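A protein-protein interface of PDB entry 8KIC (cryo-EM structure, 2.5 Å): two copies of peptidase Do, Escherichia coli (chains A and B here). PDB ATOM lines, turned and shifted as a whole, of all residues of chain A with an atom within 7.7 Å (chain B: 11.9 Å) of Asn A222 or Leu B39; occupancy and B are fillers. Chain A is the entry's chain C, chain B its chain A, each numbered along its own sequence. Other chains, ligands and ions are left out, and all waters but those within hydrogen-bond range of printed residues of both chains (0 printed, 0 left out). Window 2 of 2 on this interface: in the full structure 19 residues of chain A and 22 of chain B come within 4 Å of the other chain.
OE1 of Glu B47 is in salt-bridge range of NH1 of Arg A163.
The side-chain amide oxygen (OD1) of Asn A220 lies within hydrogen-bond range of the backbone NH (N) of Asn A222, 3.1 Å away.
Among the printed residues, merely in contact across the chains: Arg A163 with Ala B43 (3.6 Å), Arg A163 with Pro B44 (3.99 Å), Asp A166 with Ser B41 (3.5 Å), Asp A166 with Ala B43 (3.6 Å), Phe A167 with Pro B40 (3.2 Å), Phe A167 with Ser B41 (3.6 Å), Leu A221 with Leu B39 (3.7 Å) and Asn A222 with Leu B39 (3.6 Å).
Of the printed residues of chain B, Asp A166 touches Ser B41 (3.5 Å) and Ala B43 (3.6 Å). Printed residues of chain B within 4 Å of Phe A167: Pro B40 (3.2 Å) and Ser B41 (3.6 Å). No residue of chain B comes within 4 Å of Asn A220. Asn A222 touches just one residue of chain B: Leu B39. No residue of chain B comes within 4 Å of Gly A223. Glu A224 touches none of the printed residues of chain B. Leu B39 touches just these residues of chain A: Leu A221 (3.7 Å) and Asn A222 (3.6 Å). Pro B40 touches just one residue of chain A: Phe A167 (3.2 Å). Of the printed residues of chain A, Ser B41 touches Asp A166 and Phe A167. Printed residues of chain A within 4 Å of Ala B43: Arg A163 and Asp A166. Printed residues of chain A within 4 Å of Glu B47: Arg A163 (2.5 Å). The nearest printed residue of chain A that does not touch Ala B43 is Phe A167 (6.9 Å).
Of the 9 printed residues of chain B, 6 touch a printed residue of chain A. Printed residues of chain B that touch a printed residue of chain A: Leu B39, Pro B40, Ser B41, Ala B43, Pro B44 and Glu B47. Hydrophobic or aromatic side chains of chain B that line the printed part of chain A: Leu B39, Ala B43 and Pro B44. Along chain B the printed residues that touch a printed residue of chain A span positions 39 to 47. Hydrophobic or aromatic side chains of chain A within 4 Å of the printed part of chain B: Phe A167 and Leu A221. Among the printed residues, 9 pairs touch across the chains.
Positions printed for both chains: 42 and 45. Of the 9 pairs that touch across the chains among the printed residues, none has its exchanged pair printed and touching as well.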
ATOM      1  N   LEU A  42      -9.319   4.628  21.944  1.00  0.00           N
ATOM      2  CA  LEU A  42     -10.113   5.133  23.055  1.00  0.00           C
ATOM      3  C   LEU A  42     -10.078   4.209  24.261  1.00  0.00           C
ATOM      4  O   LEU A  42     -10.732   4.499  25.264  1.00  0.00           O
ATOM      5  CB  LEU A  42     -11.568   5.339  22.621  1.00  0.00           C
ATOM      6  CG  LEU A  42     -11.833   6.144  21.352  1.00  0.00           C
ATOM      7  CD1 LEU A  42     -13.281   6.014  20.939  1.00  0.00           C
ATOM      8  CD2 LEU A  42     -11.477   7.590  21.582  1.00  0.00           C
ATOM      9  N   MET A  45      -9.077   5.595  28.085  1.00  0.00           N
ATOM     10  CA  MET A  45     -10.023   6.427  28.816  1.00  0.00           C
ATOM     11  C   MET A  45     -11.319   5.689  29.125  1.00  0.00           C
ATOM     12  O   MET A  45     -11.972   5.995  30.127  1.00  0.00           O
ATOM     13  CB  MET A  45     -10.320   7.714  28.043  1.00  0.00           C
ATOM     14  CG  MET A  45     -11.277   7.574  26.878  1.00  0.00           C
ATOM     15  SD  MET A  45     -12.929   8.175  27.301  1.00  0.00           S
ATOM     16  CE  MET A  45     -13.779   7.980  25.740  1.00  0.00           C
ATOM     17  N   LEU A  46     -11.708   4.719  28.296  1.00  0.00           N
ATOM     18  CA  LEU A  46     -12.923   3.964  28.578  1.00  0.00           C
ATOM     19  C   LEU A  46     -12.727   2.998  29.737  1.00  0.00           C
ATOM     20  O   LEU A  46     -13.707   2.540  30.329  1.00  0.00           O
ATOM     21  CB  LEU A  46     -13.382   3.209  27.332  1.00  0.00           C
ATOM     22  CG  LEU A  46     -14.177   3.984  26.280  1.00  0.00           C
ATOM     23  CD1 LEU A  46     -14.440   3.111  25.068  1.00  0.00           C
ATOM     24  CD2 LEU A  46     -15.477   4.518  26.847  1.00  0.00           C
ATOM     25  N   LYS A  48     -11.438   3.651  32.694  1.00  0.00           N
ATOM     26  CA  LYS A  48     -11.746   4.324  33.948  1.00  0.00           C
ATOM     27  C   LYS A  48     -13.198   4.772  34.062  1.00  0.00           C
ATOM     28  O   LYS A  48     -13.623   5.152  35.157  1.00  0.00           O
ATOM     29  CB  LYS A  48     -10.842   5.550  34.121  1.00  0.00           C
ATOM     30  CG  LYS A  48      -9.358   5.257  34.065  1.00  0.00           C
ATOM     31  CD  LYS A  48      -8.565   6.530  33.831  1.00  0.00           C
ATOM     32  CE  LYS A  48      -8.003   6.583  32.422  1.00  0.00           C
ATOM     33  NZ  LYS A  48      -8.057   7.950  31.838  1.00  0.00           N
ATOM     34  N   VAL A  49     -13.964   4.725  32.978  1.00  0.00           N
ATOM     35  CA  VAL A  49     -15.266   5.369  32.908  1.00  0.00           C
ATOM     36  C   VAL A  49     -16.402   4.354  32.831  1.00  0.00           C
ATOM     37  O   VAL A  49     -17.481   4.586  33.380  1.00  0.00           O
ATOM     38  CB  VAL A  49     -15.302   6.351  31.713  1.00  0.00           C
ATOM     39  CG1 VAL A  49     -16.697   6.507  31.154  1.00  0.00           C
ATOM     40  CG2 VAL A  49     -14.747   7.699  32.126  1.00  0.00           C
ATOM     41  N   ALA A 155     -17.835  12.168  35.960  1.00  0.00           N
ATOM     42  CA  ALA A 155     -17.656  13.611  35.991  1.00  0.00           C
ATOM     43  C   ALA A 155     -18.476  14.248  34.877  1.00  0.00           C
ATOM     44  O   ALA A 155     -18.726  13.634  33.839  1.00  0.00           O
ATOM     45  CB  ALA A 155     -16.181  13.984  35.846  1.00  0.00           C
ATOM     46  N   ALA A 157     -19.313  17.539  32.293  1.00  0.00           N
ATOM     47  CA  ALA A 157     -18.725  18.634  31.543  1.00  0.00           C
ATOM     48  C   ALA A 157     -19.767  19.707  31.242  1.00  0.00           C
ATOM     49  O   ALA A 157     -20.976  19.468  31.268  1.00  0.00           O
ATOM     50  CB  ALA A 157     -18.107  18.115  30.243  1.00  0.00           C
ATOM     51  N   ARG A 163     -19.615  22.191  20.406  1.00  0.00           N
ATOM     52  CA  ARG A 163     -19.639  22.696  19.044  1.00  0.00           C
ATOM     53  C   ARG A 163     -19.913  21.541  18.095  1.00  0.00           C
ATOM     54  O   ARG A 163     -19.677  20.379  18.427  1.00  0.00           O
ATOM     55  CB  ARG A 163     -18.319  23.379  18.674  1.00  0.00           C
ATOM     56  CG  ARG A 163     -18.243  24.834  19.075  1.00  0.00           C
ATOM     57  CD  ARG A 163     -17.162  25.558  18.302  1.00  0.00           C
ATOM     58  NE  ARG A 163     -15.866  24.905  18.432  1.00  0.00           N
ATOM     59  CZ  ARG A 163     -14.756  25.316  17.833  1.00  0.00           C
ATOM     60  NH1 ARG A 163     -14.750  26.378  17.046  1.00  0.00           N
ATOM     61  NH2 ARG A 163     -13.627  24.642  18.028  1.00  0.00           N
ATOM     62  N   ASP A 166     -17.412  18.042  17.300  1.00  0.00           N
ATOM     63  CA  ASP A 166     -16.736  17.358  18.390  1.00  0.00           C
ATOM     64  C   ASP A 166     -17.055  15.869  18.374  1.00  0.00           C
ATOM     65  O   ASP A 166     -18.136  15.446  17.960  1.00  0.00           O
ATOM     66  CB  ASP A 166     -17.141  17.957  19.735  1.00  0.00           C
ATOM     67  CG  ASP A 166     -16.625  19.368  19.924  1.00  0.00           C
ATOM     68  OD1 ASP A 166     -15.964  19.885  19.001  1.00  0.00           O
ATOM     69  OD2 ASP A 166     -16.876  19.962  20.992  1.00  0.00           O
ATOM     70  N   PHE A 167     -16.099  15.072  18.841  1.00  0.00           N
ATOM     71  CA  PHE A 167     -16.250  13.624  18.864  1.00  0.00           C
ATOM     72  C   PHE A 167     -16.938  13.170  20.146  1.00  0.00           C
ATOM     73  O   PHE A 167     -16.735  13.748  21.216  1.00  0.00           O
ATOM     74  CB  PHE A 167     -14.884  12.955  18.725  1.00  0.00           C
ATOM     75  CG  PHE A 167     -14.184  13.279  17.442  1.00  0.00           C
ATOM     76  CD1 PHE A 167     -14.680  12.824  16.234  1.00  0.00           C
ATOM     77  CD2 PHE A 167     -13.034  14.042  17.437  1.00  0.00           C
ATOM     78  CE1 PHE A 167     -14.041  13.123  15.051  1.00  0.00           C
ATOM     79  CE2 PHE A 167     -12.393  14.342  16.256  1.00  0.00           C
ATOM     80  CZ  PHE A 167     -12.897  13.885  15.064  1.00  0.00           C
ATOM     81  N   VAL A 169     -18.812   9.595  22.365  1.00  0.00           N
ATOM     82  CA  VAL A 169     -18.945   8.158  22.589  1.00  0.00           C
ATOM     83  C   VAL A 169     -20.251   7.913  23.330  1.00  0.00           C
ATOM     84  O   VAL A 169     -20.520   8.560  24.345  1.00  0.00           O
ATOM     85  CB  VAL A 169     -17.758   7.582  23.384  1.00  0.00           C
ATOM     86  CG1 VAL A 169     -17.844   6.072  23.456  1.00  0.00           C
ATOM     87  CG2 VAL A 169     -16.444   7.998  22.763  1.00  0.00           C
ATOM     88  N   LEU A 219     -20.430  10.814  26.119  1.00  0.00           N
ATOM     89  CA  LEU A 219     -19.187  11.310  26.686  1.00  0.00           C
ATOM     90  C   LEU A 219     -18.312  11.928  25.607  1.00  0.00           C
ATOM     91  O   LEU A 219     -18.448  11.630  24.420  1.00  0.00           O
ATOM     92  CB  LEU A 219     -18.404  10.191  27.385  1.00  0.00           C
ATOM     93  CG  LEU A 219     -19.167   9.236  28.301  1.00  0.00           C
ATOM     94  CD1 LEU A 219     -18.462   7.907  28.352  1.00  0.00           C
ATOM     95  CD2 LEU A 219     -19.315   9.815  29.685  1.00  0.00           C
ATOM     96  N   ASN A 220     -17.409  12.799  26.040  1.00  0.00           N
ATOM     97  CA  ASN A 220     -16.402  13.370  25.163  1.00  0.00           C
ATOM     98  C   ASN A 220     -15.136  12.513  25.226  1.00  0.00           C
ATOM     99  O   ASN A 220     -15.139  11.407  25.768  1.00  0.00           O
ATOM    100  CB  ASN A 220     -16.154  14.836  25.518  1.00  0.00           C
ATOM    101  CG  ASN A 220     -15.673  15.036  26.942  1.00  0.00           C
ATOM    102  OD1 ASN A 220     -15.212  14.110  27.595  1.00  0.00           O
ATOM    103  ND2 ASN A 220     -15.766  16.264  27.422  1.00  0.00           N
ATOM    104  N   LEU A 221     -14.035  13.013  24.667  1.00  0.00           N
ATOM    105  CA  LEU A 221     -12.809  12.224  24.618  1.00  0.00           C
ATOM    106  C   LEU A 221     -12.080  12.164  25.954  1.00  0.00           C
ATOM    107  O   LEU A 221     -11.168  11.347  26.098  1.00  0.00           O
ATOM    108  CB  LEU A 221     -11.872  12.773  23.542  1.00  0.00           C
ATOM    109  CG  LEU A 221     -12.305  12.558  22.091  1.00  0.00           C
ATOM    110  CD1 LEU A 221     -11.201  12.957  21.134  1.00  0.00           C
ATOM    111  CD2 LEU A 221     -12.719  11.121  21.857  1.00  0.00           C
ATOM    112  N   ASN A 222     -12.452  12.993  26.924  1.00  0.00           N
ATOM    113  CA  ASN A 222     -11.887  12.925  28.266  1.00  0.00           C
ATOM    114  C   ASN A 222     -12.701  12.045  29.205  1.00  0.00           C
ATOM    115  O   ASN A 222     -12.300  11.862  30.358  1.00  0.00           O
ATOM    116  CB  ASN A 222     -11.771  14.326  28.865  1.00  0.00           C
ATOM    117  CG  ASN A 222     -10.694  15.155  28.208  1.00  0.00           C
ATOM    118  OD1 ASN A 222      -9.654  14.638  27.803  1.00  0.00           O
ATOM    119  ND2 ASN A 222     -10.934  16.456  28.103  1.00  0.00           N
ATOM    120  N   GLY A 223     -13.826  11.504  28.747  1.00  0.00           N
ATOM    121  CA  GLY A 223     -14.654  10.676  29.597  1.00  0.00           C
ATOM    122  C   GLY A 223     -15.569  11.435  30.522  1.00  0.00           C
ATOM    123  O   GLY A 223     -15.871  10.953  31.616  1.00  0.00           O
ATOM    124  N   GLU A 224     -16.017  12.618  30.120  1.00  0.00           N
ATOM    125  CA  GLU A 224     -16.916  13.434  30.919  1.00  0.00           C
ATOM    126  C   GLU A 224     -18.302  13.447  30.293  1.00  0.00           C
ATOM    127  O   GLU A 224     -18.441  13.405  29.070  1.00  0.00           O
ATOM    128  CB  GLU A 224     -16.378  14.855  31.049  1.00  0.00           C
ATOM    129  CG  GLU A 224     -15.578  15.067  32.302  1.00  0.00           C
ATOM    130  CD  GLU A 224     -14.478  16.079  32.122  1.00  0.00           C
ATOM    131  OE1 GLU A 224     -14.221  16.855  33.066  1.00  0.00           O
ATOM    132  OE2 GLU A 224     -13.859  16.090  31.040  1.00  0.00           O
ATOM    133  N   LEU A 225     -19.322  13.502  31.143  1.00  0.00           N
ATOM    134  CA  LEU A 225     -20.697  13.416  30.679  1.00  0.00           C
ATOM    135  C   LEU A 225     -21.102  14.694  29.957  1.00  0.00           C
ATOM    136  O   LEU A 225     -20.924  15.796  30.479  1.00  0.00           O
ATOM    137  CB  LEU A 225     -21.622  13.159  31.868  1.00  0.00           C
ATOM    138  CG  LEU A 225     -23.076  12.766  31.622  1.00  0.00           C
ATOM    139  CD1 LEU A 225     -23.173  11.337  31.142  1.00  0.00           C
ATOM    140  CD2 LEU A 225     -23.876  12.951  32.888  1.00  0.00           C
ATOM    141  N   PRO B  38      -7.079  21.728  22.291  1.00  0.00           N
ATOM    142  CA  PRO B  38      -6.508  20.543  22.931  1.00  0.00           C
ATOM    143  C   PRO B  38      -7.059  19.237  22.364  1.00  0.00           C
ATOM    144  O   PRO B  38      -6.316  18.486  21.733  1.00  0.00           O
ATOM    145  CB  PRO B  38      -6.913  20.713  24.400  1.00  0.00           C
ATOM    146  CG  PRO B  38      -7.211  22.196  24.572  1.00  0.00           C
ATOM    147  CD  PRO B  38      -7.156  22.864  23.223  1.00  0.00           C
ATOM    148  N   LEU B  39      -8.342  18.972  22.596  1.00  0.00           N
ATOM    149  CA  LEU B  39      -8.951  17.758  22.078  1.00  0.00           C
ATOM    150  C   LEU B  39      -9.122  17.861  20.563  1.00  0.00           C
ATOM    151  O   LEU B  39      -9.510  18.917  20.054  1.00  0.00           O
ATOM    152  CB  LEU B  39     -10.309  17.514  22.738  1.00  0.00           C
ATOM    153  CG  LEU B  39     -10.327  16.837  24.112  1.00  0.00           C
ATOM    154  CD1 LEU B  39     -11.758  16.585  24.568  1.00  0.00           C
ATOM    155  CD2 LEU B  39      -9.527  15.544  24.103  1.00  0.00           C
ATOM    156  N   PRO B  40      -8.838  16.792  19.820  1.00  0.00           N
ATOM    157  CA  PRO B  40      -9.097  16.812  18.374  1.00  0.00           C
ATOM    158  C   PRO B  40     -10.581  16.972  18.079  1.00  0.00           C
ATOM    159  O   PRO B  40     -11.435  16.453  18.798  1.00  0.00           O
ATOM    160  CB  PRO B  40      -8.575  15.452  17.898  1.00  0.00           C
ATOM    161  CG  PRO B  40      -7.699  14.953  18.987  1.00  0.00           C
ATOM    162  CD  PRO B  40      -8.200  15.543  20.260  1.00  0.00           C
ATOM    163  N   SER B  41     -10.883  17.702  17.008  1.00  0.00           N
ATOM    164  CA  SER B  41     -12.262  17.883  16.582  1.00  0.00           C
ATOM    165  C   SER B  41     -12.281  18.344  15.136  1.00  0.00           C
ATOM    166  O   SER B  41     -11.281  18.831  14.605  1.00  0.00           O
ATOM    167  CB  SER B  41     -13.005  18.889  17.467  1.00  0.00           C
ATOM    168  OG  SER B  41     -12.148  19.935  17.875  1.00  0.00           O
ATOM    169  N   LEU B  42     -13.437  18.172  14.505  1.00  0.00           N
ATOM    170  CA  LEU B  42     -13.717  18.752  13.202  1.00  0.00           C
ATOM    171  C   LEU B  42     -14.347  20.130  13.306  1.00  0.00           C
ATOM    172  O   LEU B  42     -14.652  20.735  12.279  1.00  0.00           O
ATOM    173  CB  LEU B  42     -14.638  17.828  12.400  1.00  0.00           C
ATOM    174  CG  LEU B  42     -14.198  16.378  12.216  1.00  0.00           C
ATOM    175  CD1 LEU B  42     -15.314  15.568  11.596  1.00  0.00           C
ATOM    176  CD2 LEU B  42     -12.948  16.310  11.361  1.00  0.00           C
ATOM    177  N   ALA B  43     -14.557  20.627  14.523  1.00  0.00           N
ATOM    178  CA  ALA B  43     -15.209  21.919  14.703  1.00  0.00           C
ATOM    179  C   ALA B  43     -14.449  23.099  14.103  1.00  0.00           C
ATOM    180  O   ALA B  43     -15.106  23.969  13.505  1.00  0.00           O
ATOM    181  CB  ALA B  43     -15.477  22.147  16.195  1.00  0.00           C
ATOM    182  N   PRO B  44     -13.123  23.228  14.243  1.00  0.00           N
ATOM    183  CA  PRO B  44     -12.453  24.402  13.660  1.00  0.00           C
ATOM    184  C   PRO B  44     -12.623  24.541  12.156  1.00  0.00           C
ATOM    185  O   PRO B  44     -12.737  25.670  11.664  1.00  0.00           O
ATOM    186  CB  PRO B  44     -10.982  24.182  14.038  1.00  0.00           C
ATOM    187  CG  PRO B  44     -11.037  23.355  15.250  1.00  0.00           C
ATOM    188  CD  PRO B  44     -12.180  22.424  15.041  1.00  0.00           C
ATOM    189  N   MET B  45     -12.638  23.441  11.407  1.00  0.00           N
ATOM    190  CA  MET B  45     -12.763  23.532   9.958  1.00  0.00           C
ATOM    191  C   MET B  45     -14.211  23.577   9.491  1.00  0.00           C
ATOM    192  O   MET B  45     -14.487  24.124   8.420  1.00  0.00           O
ATOM    193  CB  MET B  45     -12.023  22.367   9.288  1.00  0.00           C
ATOM    194  CG  MET B  45     -12.836  21.107   9.065  1.00  0.00           C
ATOM    195  SD  MET B  45     -13.612  21.008   7.443  1.00  0.00           S
ATOM    196  CE  MET B  45     -14.654  19.572   7.654  1.00  0.00           C
ATOM    197  N   GLU B  47     -16.547  25.281  10.995  1.00  0.00           N
ATOM    198  CA  GLU B  47     -17.097  26.599  11.283  1.00  0.00           C
ATOM    199  C   GLU B  47     -16.974  27.545  10.095  1.00  0.00           C
ATOM    200  O   GLU B  47     -17.691  28.548  10.025  1.00  0.00           O
ATOM    201  CB  GLU B  47     -16.402  27.192  12.509  1.00  0.00           C
ATOM    202  CG  GLU B  47     -17.286  28.100  13.341  1.00  0.00           C
ATOM    203  CD  GLU B  47     -17.084  27.907  14.834  1.00  0.00           C
ATOM    204  OE1 GLU B  47     -16.315  27.003  15.224  1.00  0.00           O
ATOM    205  OE2 GLU B  47     -17.692  28.661  15.621  1.00  0.00           O
